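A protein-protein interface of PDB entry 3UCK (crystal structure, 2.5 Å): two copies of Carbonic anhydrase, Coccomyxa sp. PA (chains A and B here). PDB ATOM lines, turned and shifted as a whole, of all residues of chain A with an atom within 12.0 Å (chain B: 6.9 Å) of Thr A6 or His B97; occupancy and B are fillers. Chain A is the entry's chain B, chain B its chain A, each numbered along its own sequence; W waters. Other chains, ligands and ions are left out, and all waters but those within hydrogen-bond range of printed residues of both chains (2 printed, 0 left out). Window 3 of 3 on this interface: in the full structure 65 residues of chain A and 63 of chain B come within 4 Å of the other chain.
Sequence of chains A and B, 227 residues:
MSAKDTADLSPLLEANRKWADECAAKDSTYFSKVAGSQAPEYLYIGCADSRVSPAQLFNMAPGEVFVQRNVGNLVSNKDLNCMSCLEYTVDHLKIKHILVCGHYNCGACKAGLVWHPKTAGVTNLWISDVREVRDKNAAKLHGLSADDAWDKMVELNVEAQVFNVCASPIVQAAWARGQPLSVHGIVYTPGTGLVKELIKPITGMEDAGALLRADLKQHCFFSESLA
N of Leu B43 is in hydrogen-bond range of O of His B97 (2.8 Å).
N of Ser B182 is in hydrogen-bond range of O of Lys B96.
ND1 of His B97 sits at hydrogen-bond distance from OG of Ser B182 (2.9 Å).
O of Ser B182 sits at hydrogen-bond distance from N of Ile B98 (2.7 Å).
The backbone carbonyl oxygen of Ile B98 is in hydrogen-bond range of the backbone NH of His B184, 2.9 Å away.
A ring nitrogen (NE2) of His B184 lies within hydrogen-bond range of the side-chain hydroxyl (OG) of Ser B182 (2.6 Å).
Among the printed residues, merely in contact across the chains: Leu A12 with Tyr B42 (2.9 Å), Ser A50 with Val B65 (3.3 Å), Ala A7 with His B184 (3.4 Å), Leu A9 with His B184 (3.5 Å), Thr A6 with His B97 (3.6 Å) and Ala A7 with Ser B182 (3.8 Å).
Printed residues of chain B within 4 Å of Ala A7: Ser B182 and His B184.
Printed residues of chain B within 4 Å of Leu A9: His B184 (3.5 Å).
Ala A48 touches none of the printed residues of chain B.
Printed residues of chain B within 4 Å of Ser A50: Val B65 (3.3 Å).
Tyr B42 touches one residue of chain A.
Leu B43 touches none of the printed residues of chain A.
Printed residues of chain A within 4 Å of Val B65: Ser A50 (3.3 Å).
Lys B94 touches none of the printed residues of chain A.
No residue of chain A comes within 4 Å of Ile B98.
No residue of chain A comes within 4 Å of Leu B99.
No residue of chain A comes within 4 Å of Leu B181.
Printed residues of chain A within 4 Å of Ser B182: Ala A7.
Of the printed residues of chain A, His B184 touches Ala A7 and Leu A9.
The nearest residue of chain A that does not touch His B97 is Ala A7 (4.2 Å).
The nearest printed residue of chain A that does not touch His B184 is Asp A8 (4.9 Å).
Hydrophobic or aromatic side chains of chain A within 4 Å of the printed part of chain B: Ala A7, Leu A9 and Leu A12.
Among the printed residues, 6 pairs touch across the chains.
No position is printed for both chains.
Of the 6 pairs that touch across the chains among the printed residues, none has its exchanged pair printed and touching as well.
Water W1 lies within hydrogen-bond range of O of Val B65 (2.7 Å) and O of Ser A50 (3.3 Å).
Water W2 bridges the backbone carbonyl oxygen (O) of Ser A50 (2.7 Å) and the backbone NH (N) of Val B65 (2.9 Å).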
ATOM      1  N   THR A   6     -19.748 -14.838  -6.486  1.00  0.00           N
ATOM      2  CA  THR A   6     -19.702 -15.361  -5.128  1.00  0.00           C
ATOM      3  C   THR A   6     -20.748 -14.684  -4.256  1.00  0.00           C
ATOM      4  O   THR A   6     -20.915 -13.478  -4.322  1.00  0.00           O
ATOM      5  CB  THR A   6     -18.314 -15.175  -4.523  1.00  0.00           C
ATOM      6  OG1 THR A   6     -18.404 -15.167  -3.105  1.00  0.00           O
ATOM      7  CG2 THR A   6     -17.736 -13.879  -4.970  1.00  0.00           C
ATOM      8  N   ALA A   7     -21.447 -15.459  -3.436  1.00  0.00           N
ATOM      9  CA  ALA A   7     -22.543 -14.906  -2.659  1.00  0.00           C
ATOM     10  C   ALA A   7     -22.469 -15.044  -1.139  1.00  0.00           C
ATOM     11  O   ALA A   7     -23.428 -14.765  -0.463  1.00  0.00           O
ATOM     12  CB  ALA A   7     -23.843 -15.452  -3.164  1.00  0.00           C
ATOM     13  N   ASP A   8     -21.348 -15.452  -0.589  1.00  0.00           N
ATOM     14  CA  ASP A   8     -21.272 -15.522   0.854  1.00  0.00           C
ATOM     15  C   ASP A   8     -21.755 -14.214   1.405  1.00  0.00           C
ATOM     16  O   ASP A   8     -22.030 -13.320   0.651  1.00  0.00           O
ATOM     17  CB  ASP A   8     -19.855 -15.783   1.311  1.00  0.00           C
ATOM     18  CG  ASP A   8     -19.806 -16.454   2.635  1.00  0.00           C
ATOM     19  OD1 ASP A   8     -19.886 -17.685   2.680  1.00  0.00           O
ATOM     20  OD2 ASP A   8     -19.698 -15.754   3.640  1.00  0.00           O
ATOM     21  N   LEU A   9     -21.844 -14.100   2.721  1.00  0.00           N
ATOM     22  CA  LEU A   9     -22.498 -12.971   3.371  1.00  0.00           C
ATOM     23  C   LEU A   9     -21.884 -12.562   4.692  1.00  0.00           C
ATOM     24  O   LEU A   9     -22.444 -11.751   5.394  1.00  0.00           O
ATOM     25  CB  LEU A   9     -23.926 -13.363   3.701  1.00  0.00           C
ATOM     26  CG  LEU A   9     -25.178 -12.976   2.926  1.00  0.00           C
ATOM     27  CD1 LEU A   9     -26.275 -12.797   3.925  1.00  0.00           C
ATOM     28  CD2 LEU A   9     -25.005 -11.737   2.137  1.00  0.00           C
ATOM     29  N   SER A  10     -20.758 -13.141   5.063  1.00  0.00           N
ATOM     30  CA  SER A  10     -20.211 -12.906   6.386  1.00  0.00           C
ATOM     31  C   SER A  10     -19.524 -11.580   6.427  1.00  0.00           C
ATOM     32  O   SER A  10     -19.671 -10.793   7.348  1.00  0.00           O
ATOM     33  CB  SER A  10     -19.230 -14.002   6.714  1.00  0.00           C
ATOM     34  OG  SER A  10     -19.372 -15.064   5.803  1.00  0.00           O
ATOM     35  N   PRO A  11     -18.766 -11.332   5.391  1.00  0.00           N
ATOM     36  CA  PRO A  11     -18.210 -10.015   5.200  1.00  0.00           C
ATOM     37  C   PRO A  11     -19.227  -9.062   5.736  1.00  0.00           C
ATOM     38  O   PRO A  11     -19.041  -8.501   6.787  1.00  0.00           O
ATOM     39  CB  PRO A  11     -18.132  -9.908   3.692  1.00  0.00           C
ATOM     40  CG  PRO A  11     -17.940 -11.273   3.253  1.00  0.00           C
ATOM     41  CD  PRO A  11     -18.752 -12.119   4.159  1.00  0.00           C
ATOM     42  N   LEU A  12     -20.323  -8.915   5.016  1.00  0.00           N
ATOM     43  CA  LEU A  12     -21.404  -8.055   5.422  1.00  0.00           C
ATOM     44  C   LEU A  12     -21.776  -8.295   6.851  1.00  0.00           C
ATOM     45  O   LEU A  12     -21.765  -7.411   7.666  1.00  0.00           O
ATOM     46  CB  LEU A  12     -22.612  -8.323   4.552  1.00  0.00           C
ATOM     47  CG  LEU A  12     -23.177  -7.099   3.837  1.00  0.00           C
ATOM     48  CD1 LEU A  12     -23.708  -7.490   2.502  1.00  0.00           C
ATOM     49  CD2 LEU A  12     -24.258  -6.461   4.641  1.00  0.00           C
ATOM     50  N   LEU A  13     -22.103  -9.525   7.154  1.00  0.00           N
ATOM     51  CA  LEU A  13     -22.495  -9.868   8.495  1.00  0.00           C
ATOM     52  C   LEU A  13     -21.487  -9.409   9.502  1.00  0.00           C
ATOM     53  O   LEU A  13     -21.830  -9.161  10.641  1.00  0.00           O
ATOM     54  CB  LEU A  13     -22.675 -11.357   8.606  1.00  0.00           C
ATOM     55  CG  LEU A  13     -23.994 -11.788   8.019  1.00  0.00           C
ATOM     56  CD1 LEU A  13     -24.021 -13.271   7.942  1.00  0.00           C
ATOM     57  CD2 LEU A  13     -25.083 -11.281   8.901  1.00  0.00           C
ATOM     58  N   ALA A  48     -36.059   5.016  -3.810  1.00  0.00           N
ATOM     59  CA  ALA A  48     -35.361   3.814  -3.479  1.00  0.00           C
ATOM     60  C   ALA A  48     -33.909   3.829  -3.944  1.00  0.00           C
ATOM     61  O   ALA A  48     -33.194   2.911  -3.687  1.00  0.00           O
ATOM     62  CB  ALA A  48     -36.074   2.657  -4.065  1.00  0.00           C
ATOM     63  N   SER A  50     -30.044   4.026  -4.361  1.00  0.00           N
ATOM     64  CA  SER A  50     -28.946   3.596  -3.421  1.00  0.00           C
ATOM     65  C   SER A  50     -28.153   4.686  -2.779  1.00  0.00           C
ATOM     66  O   SER A  50     -27.423   4.435  -1.819  1.00  0.00           O
ATOM     67  CB  SER A  50     -27.935   2.736  -4.154  1.00  0.00           C
ATOM     68  OG  SER A  50     -27.572   3.350  -5.355  1.00  0.00           O
ATOM     69  N   GLU B  41     -24.709  -3.012  -5.610  1.00  0.00           N
ATOM     70  CA  GLU B  41     -24.628  -4.431  -5.790  1.00  0.00           C
ATOM     71  C   GLU B  41     -25.824  -5.119  -5.188  1.00  0.00           C
ATOM     72  O   GLU B  41     -26.232  -6.153  -5.648  1.00  0.00           O
ATOM     73  CB  GLU B  41     -23.360  -4.942  -5.134  1.00  0.00           C
ATOM     74  CG  GLU B  41     -22.101  -4.416  -5.768  1.00  0.00           C
ATOM     75  CD  GLU B  41     -21.013  -5.449  -5.867  1.00  0.00           C
ATOM     76  OE1 GLU B  41     -20.637  -5.804  -6.993  1.00  0.00           O
ATOM     77  OE2 GLU B  41     -20.537  -5.897  -4.816  1.00  0.00           O
ATOM     78  N   TYR B  42     -26.367  -4.514  -4.145  1.00  0.00           N
ATOM     79  CA  TYR B  42     -27.472  -5.049  -3.378  1.00  0.00           C
ATOM     80  C   TYR B  42     -28.795  -4.353  -3.599  1.00  0.00           C
ATOM     81  O   TYR B  42     -28.851  -3.170  -3.785  1.00  0.00           O
ATOM     82  CB  TYR B  42     -27.173  -4.900  -1.906  1.00  0.00           C
ATOM     83  CG  TYR B  42     -25.987  -5.647  -1.455  1.00  0.00           C
ATOM     84  CD1 TYR B  42     -26.117  -6.802  -0.737  1.00  0.00           C
ATOM     85  CD2 TYR B  42     -24.731  -5.217  -1.758  1.00  0.00           C
ATOM     86  CE1 TYR B  42     -25.036  -7.497  -0.320  1.00  0.00           C
ATOM     87  CE2 TYR B  42     -23.644  -5.911  -1.348  1.00  0.00           C
ATOM     88  CZ  TYR B  42     -23.802  -7.046  -0.629  1.00  0.00           C
ATOM     89  OH  TYR B  42     -22.718  -7.740  -0.223  1.00  0.00           O
ATOM     90  N   LEU B  43     -29.862  -5.127  -3.538  1.00  0.00           N
ATOM     91  CA  LEU B  43     -31.198  -4.624  -3.342  1.00  0.00           C
ATOM     92  C   LEU B  43     -31.653  -5.101  -2.000  1.00  0.00           C
ATOM     93  O   LEU B  43     -31.523  -6.241  -1.703  1.00  0.00           O
ATOM     94  CB  LEU B  43     -32.149  -5.177  -4.373  1.00  0.00           C
ATOM     95  CG  LEU B  43     -33.592  -5.072  -3.890  1.00  0.00           C
ATOM     96  CD1 LEU B  43     -33.913  -3.670  -3.583  1.00  0.00           C
ATOM     97  CD2 LEU B  43     -34.543  -5.585  -4.906  1.00  0.00           C
ATOM     98  N   TYR B  44     -32.194  -4.216  -1.196  1.00  0.00           N
ATOM     99  CA  TYR B  44     -32.688  -4.588   0.101  1.00  0.00           C
ATOM    100  C   TYR B  44     -34.152  -4.306   0.171  1.00  0.00           C
ATOM    101  O   TYR B  44     -34.600  -3.245  -0.173  1.00  0.00           O
ATOM    102  CB  TYR B  44     -31.926  -3.835   1.176  1.00  0.00           C
ATOM    103  CG  TYR B  44     -32.486  -3.825   2.567  1.00  0.00           C
ATOM    104  CD1 TYR B  44     -31.880  -4.514   3.575  1.00  0.00           C
ATOM    105  CD2 TYR B  44     -33.582  -3.076   2.881  1.00  0.00           C
ATOM    106  CE1 TYR B  44     -32.370  -4.475   4.830  1.00  0.00           C
ATOM    107  CE2 TYR B  44     -34.064  -3.031   4.129  1.00  0.00           C
ATOM    108  CZ  TYR B  44     -33.465  -3.725   5.099  1.00  0.00           C
ATOM    109  OH  TYR B  44     -33.985  -3.670   6.331  1.00  0.00           O
ATOM    110  N   VAL B  65     -26.474   0.146  -1.742  1.00  0.00           N
ATOM    111  CA  VAL B  65     -27.698  -0.644  -1.538  1.00  0.00           C
ATOM    112  C   VAL B  65     -28.945   0.146  -1.870  1.00  0.00           C
ATOM    113  O   VAL B  65     -29.265   1.126  -1.203  1.00  0.00           O
ATOM    114  CB  VAL B  65     -27.795  -1.217  -0.121  1.00  0.00           C
ATOM    115  CG1 VAL B  65     -27.936  -0.094   0.933  1.00  0.00           C
ATOM    116  CG2 VAL B  65     -28.971  -2.142  -0.036  1.00  0.00           C
ATOM    117  N   LYS B  94     -28.604  -4.151 -12.868  1.00  0.00           N
ATOM    118  CA  LYS B  94     -27.954  -5.462 -12.737  1.00  0.00           C
ATOM    119  C   LYS B  94     -27.351  -5.730 -11.356  1.00  0.00           C
ATOM    120  O   LYS B  94     -26.184  -6.101 -11.296  1.00  0.00           O
ATOM    121  CB  LYS B  94     -26.834  -5.614 -13.810  1.00  0.00           C
ATOM    122  CG  LYS B  94     -27.224  -6.333 -15.094  1.00  0.00           C
ATOM    123  CD  LYS B  94     -28.203  -5.518 -15.964  1.00  0.00           C
ATOM    124  CE  LYS B  94     -27.496  -4.729 -17.102  1.00  0.00           C
ATOM    125  NZ  LYS B  94     -26.864  -5.644 -18.133  1.00  0.00           N
ATOM    126  N   ILE B  95     -28.095  -5.552 -10.256  1.00  0.00           N
ATOM    127  CA  ILE B  95     -27.550  -5.849  -8.913  1.00  0.00           C
ATOM    128  C   ILE B  95     -27.247  -7.354  -8.836  1.00  0.00           C
ATOM    129  O   ILE B  95     -27.732  -8.114  -9.676  1.00  0.00           O
ATOM    130  CB  ILE B  95     -28.509  -5.478  -7.733  1.00  0.00           C
ATOM    131  CG1 ILE B  95     -29.862  -6.123  -7.920  1.00  0.00           C
ATOM    132  CG2 ILE B  95     -28.666  -4.007  -7.539  1.00  0.00           C
ATOM    133  CD1 ILE B  95     -30.202  -6.868  -6.736  1.00  0.00           C
ATOM    134  N   LYS B  96     -26.469  -7.775  -7.828  1.00  0.00           N
ATOM    135  CA  LYS B  96     -26.061  -9.211  -7.647  1.00  0.00           C
ATOM    136  C   LYS B  96     -26.824  -9.913  -6.524  1.00  0.00           C
ATOM    137  O   LYS B  96     -27.166 -11.093  -6.622  1.00  0.00           O
ATOM    138  CB  LYS B  96     -24.527  -9.336  -7.399  1.00  0.00           C
ATOM    139  CG  LYS B  96     -23.647  -9.117  -8.701  1.00  0.00           C
ATOM    140  CD  LYS B  96     -22.139  -9.498  -8.540  1.00  0.00           C
ATOM    141  CE  LYS B  96     -21.223  -8.475  -9.248  1.00  0.00           C
ATOM    142  NZ  LYS B  96     -19.772  -8.681  -8.868  1.00  0.00           N
ATOM    143  N   HIS B  97     -27.099  -9.159  -5.466  1.00  0.00           N
ATOM    144  CA  HIS B  97     -27.661  -9.704  -4.242  1.00  0.00           C
ATOM    145  C   HIS B  97     -28.995  -9.049  -3.784  1.00  0.00           C
ATOM    146  O   HIS B  97     -29.099  -7.810  -3.734  1.00  0.00           O
ATOM    147  CB  HIS B  97     -26.596  -9.586  -3.139  1.00  0.00           C
ATOM    148  CG  HIS B  97     -25.241 -10.057  -3.572  1.00  0.00           C
ATOM    149  ND1 HIS B  97     -25.052 -11.204  -4.325  1.00  0.00           N
ATOM    150  CD2 HIS B  97     -24.004  -9.546  -3.347  1.00  0.00           C
ATOM    151  CE1 HIS B  97     -23.763 -11.368  -4.552  1.00  0.00           C
ATOM    152  NE2 HIS B  97     -23.105 -10.382  -3.962  1.00  0.00           N
ATOM    153  N   ILE B  98     -29.981  -9.873  -3.417  1.00  0.00           N
ATOM    154  CA  ILE B  98     -31.250  -9.355  -2.902  1.00  0.00           C
ATOM    155  C   ILE B  98     -31.373  -9.714  -1.440  1.00  0.00           C
ATOM    156  O   ILE B  98     -31.457 -10.862  -1.088  1.00  0.00           O
ATOM    157  CB  ILE B  98     -32.471  -9.874  -3.705  1.00  0.00           C
ATOM    158  CG1 ILE B  98     -32.342  -9.460  -5.179  1.00  0.00           C
ATOM    159  CG2 ILE B  98     -33.788  -9.286  -3.089  1.00  0.00           C
ATOM    160  CD1 ILE B  98     -33.223 -10.202  -6.169  1.00  0.00           C
ATOM    161  N   LEU B  99     -31.358  -8.733  -0.583  1.00  0.00           N
ATOM    162  CA  LEU B  99     -31.560  -8.976   0.821  1.00  0.00           C
ATOM    163  C   LEU B  99     -33.050  -8.818   1.209  1.00  0.00           C
ATOM    164  O   LEU B  99     -33.633  -7.708   1.112  1.00  0.00           O
ATOM    165  CB  LEU B  99     -30.716  -8.002   1.641  1.00  0.00           C
ATOM    166  CG  LEU B  99     -29.224  -7.942   1.264  1.00  0.00           C
ATOM    167  CD1 LEU B  99     -28.551  -6.762   1.970  1.00  0.00           C
ATOM    168  CD2 LEU B  99     -28.537  -9.271   1.623  1.00  0.00           C
ATOM    169  N   PRO B 180     -26.331 -13.725 -12.832  1.00  0.00           N
ATOM    170  CA  PRO B 180     -26.154 -14.122 -11.433  1.00  0.00           C
ATOM    171  C   PRO B 180     -26.909 -13.206 -10.492  1.00  0.00           C
ATOM    172  O   PRO B 180     -26.690 -11.970 -10.419  1.00  0.00           O
ATOM    173  CB  PRO B 180     -24.632 -14.023 -11.184  1.00  0.00           C
ATOM    174  CG  PRO B 180     -24.104 -13.184 -12.299  1.00  0.00           C
ATOM    175  CD  PRO B 180     -25.035 -13.452 -13.485  1.00  0.00           C
ATOM    176  N   LEU B 181     -27.771 -13.851  -9.731  1.00  0.00           N
ATOM    177  CA  LEU B 181     -28.625 -13.168  -8.807  1.00  0.00           C
ATOM    178  C   LEU B 181     -28.780 -14.071  -7.623  1.00  0.00           C
ATOM    179  O   LEU B 181     -29.230 -15.211  -7.737  1.00  0.00           O
ATOM    180  CB  LEU B 181     -29.983 -12.905  -9.485  1.00  0.00           C
ATOM    181  CG  LEU B 181     -30.933 -11.972  -8.742  1.00  0.00           C
ATOM    182  CD1 LEU B 181     -30.220 -10.705  -8.334  1.00  0.00           C
ATOM    183  CD2 LEU B 181     -32.079 -11.697  -9.659  1.00  0.00           C
ATOM    184  N   SER B 182     -28.378 -13.571  -6.481  1.00  0.00           N
ATOM    185  CA  SER B 182     -28.594 -14.308  -5.282  1.00  0.00           C
ATOM    186  C   SER B 182     -29.688 -13.610  -4.422  1.00  0.00           C
ATOM    187  O   SER B 182     -29.862 -12.379  -4.486  1.00  0.00           O
ATOM    188  CB  SER B 182     -27.264 -14.483  -4.543  1.00  0.00           C
ATOM    189  OG  SER B 182     -26.952 -13.371  -3.735  1.00  0.00           O
ATOM    190  N   VAL B 183     -30.398 -14.416  -3.630  1.00  0.00           N
ATOM    191  CA  VAL B 183     -31.473 -13.976  -2.753  1.00  0.00           C
ATOM    192  C   VAL B 183     -31.244 -14.550  -1.380  1.00  0.00           C
ATOM    193  O   VAL B 183     -30.918 -15.727  -1.272  1.00  0.00           O
ATOM    194  CB  VAL B 183     -32.885 -14.421  -3.268  1.00  0.00           C
ATOM    195  CG1 VAL B 183     -33.979 -13.809  -2.390  1.00  0.00           C
ATOM    196  CG2 VAL B 183     -33.104 -14.061  -4.765  1.00  0.00           C
ATOM    197  N   HIS B 184     -31.448 -13.713  -0.351  1.00  0.00           N
ATOM    198  CA  HIS B 184     -31.030 -13.969   1.027  1.00  0.00           C
ATOM    199  C   HIS B 184     -32.098 -13.643   2.070  1.00  0.00           C
ATOM    200  O   HIS B 184     -32.571 -12.504   2.159  1.00  0.00           O
ATOM    201  CB  HIS B 184     -29.804 -13.106   1.377  1.00  0.00           C
ATOM    202  CG  HIS B 184     -28.630 -13.330   0.473  1.00  0.00           C
ATOM    203  ND1 HIS B 184     -27.624 -14.237   0.762  1.00  0.00           N
ATOM    204  CD2 HIS B 184     -28.333 -12.808  -0.742  1.00  0.00           C
ATOM    205  CE1 HIS B 184     -26.748 -14.236  -0.231  1.00  0.00           C
ATOM    206  NE2 HIS B 184     -27.165 -13.395  -1.162  1.00  0.00           N
ATOM    207  N   THR B 203     -29.071 -19.043  -5.036  1.00  0.00           N
ATOM    208  CA  THR B 203     -28.431 -18.462  -6.239  1.00  0.00           C
ATOM    209  C   THR B 203     -29.092 -18.939  -7.520  1.00  0.00           C
ATOM    210  O   THR B 203     -28.764 -18.477  -8.612  1.00  0.00           O
ATOM    211  CB  THR B 203     -26.859 -18.691  -6.345  1.00  0.00           C
ATOM    212  OG1 THR B 203     -26.593 -19.905  -7.067  1.00  0.00           O
ATOM    213  CG2 THR B 203     -26.123 -18.719  -4.972  1.00  0.00           C
HETATM  214  O   HOH W   1     -29.832   3.368   0.172  1.00  0.00           O
HETATM  215  O   HOH W   2     -26.088   2.626  -0.321  1.00  0.00           O
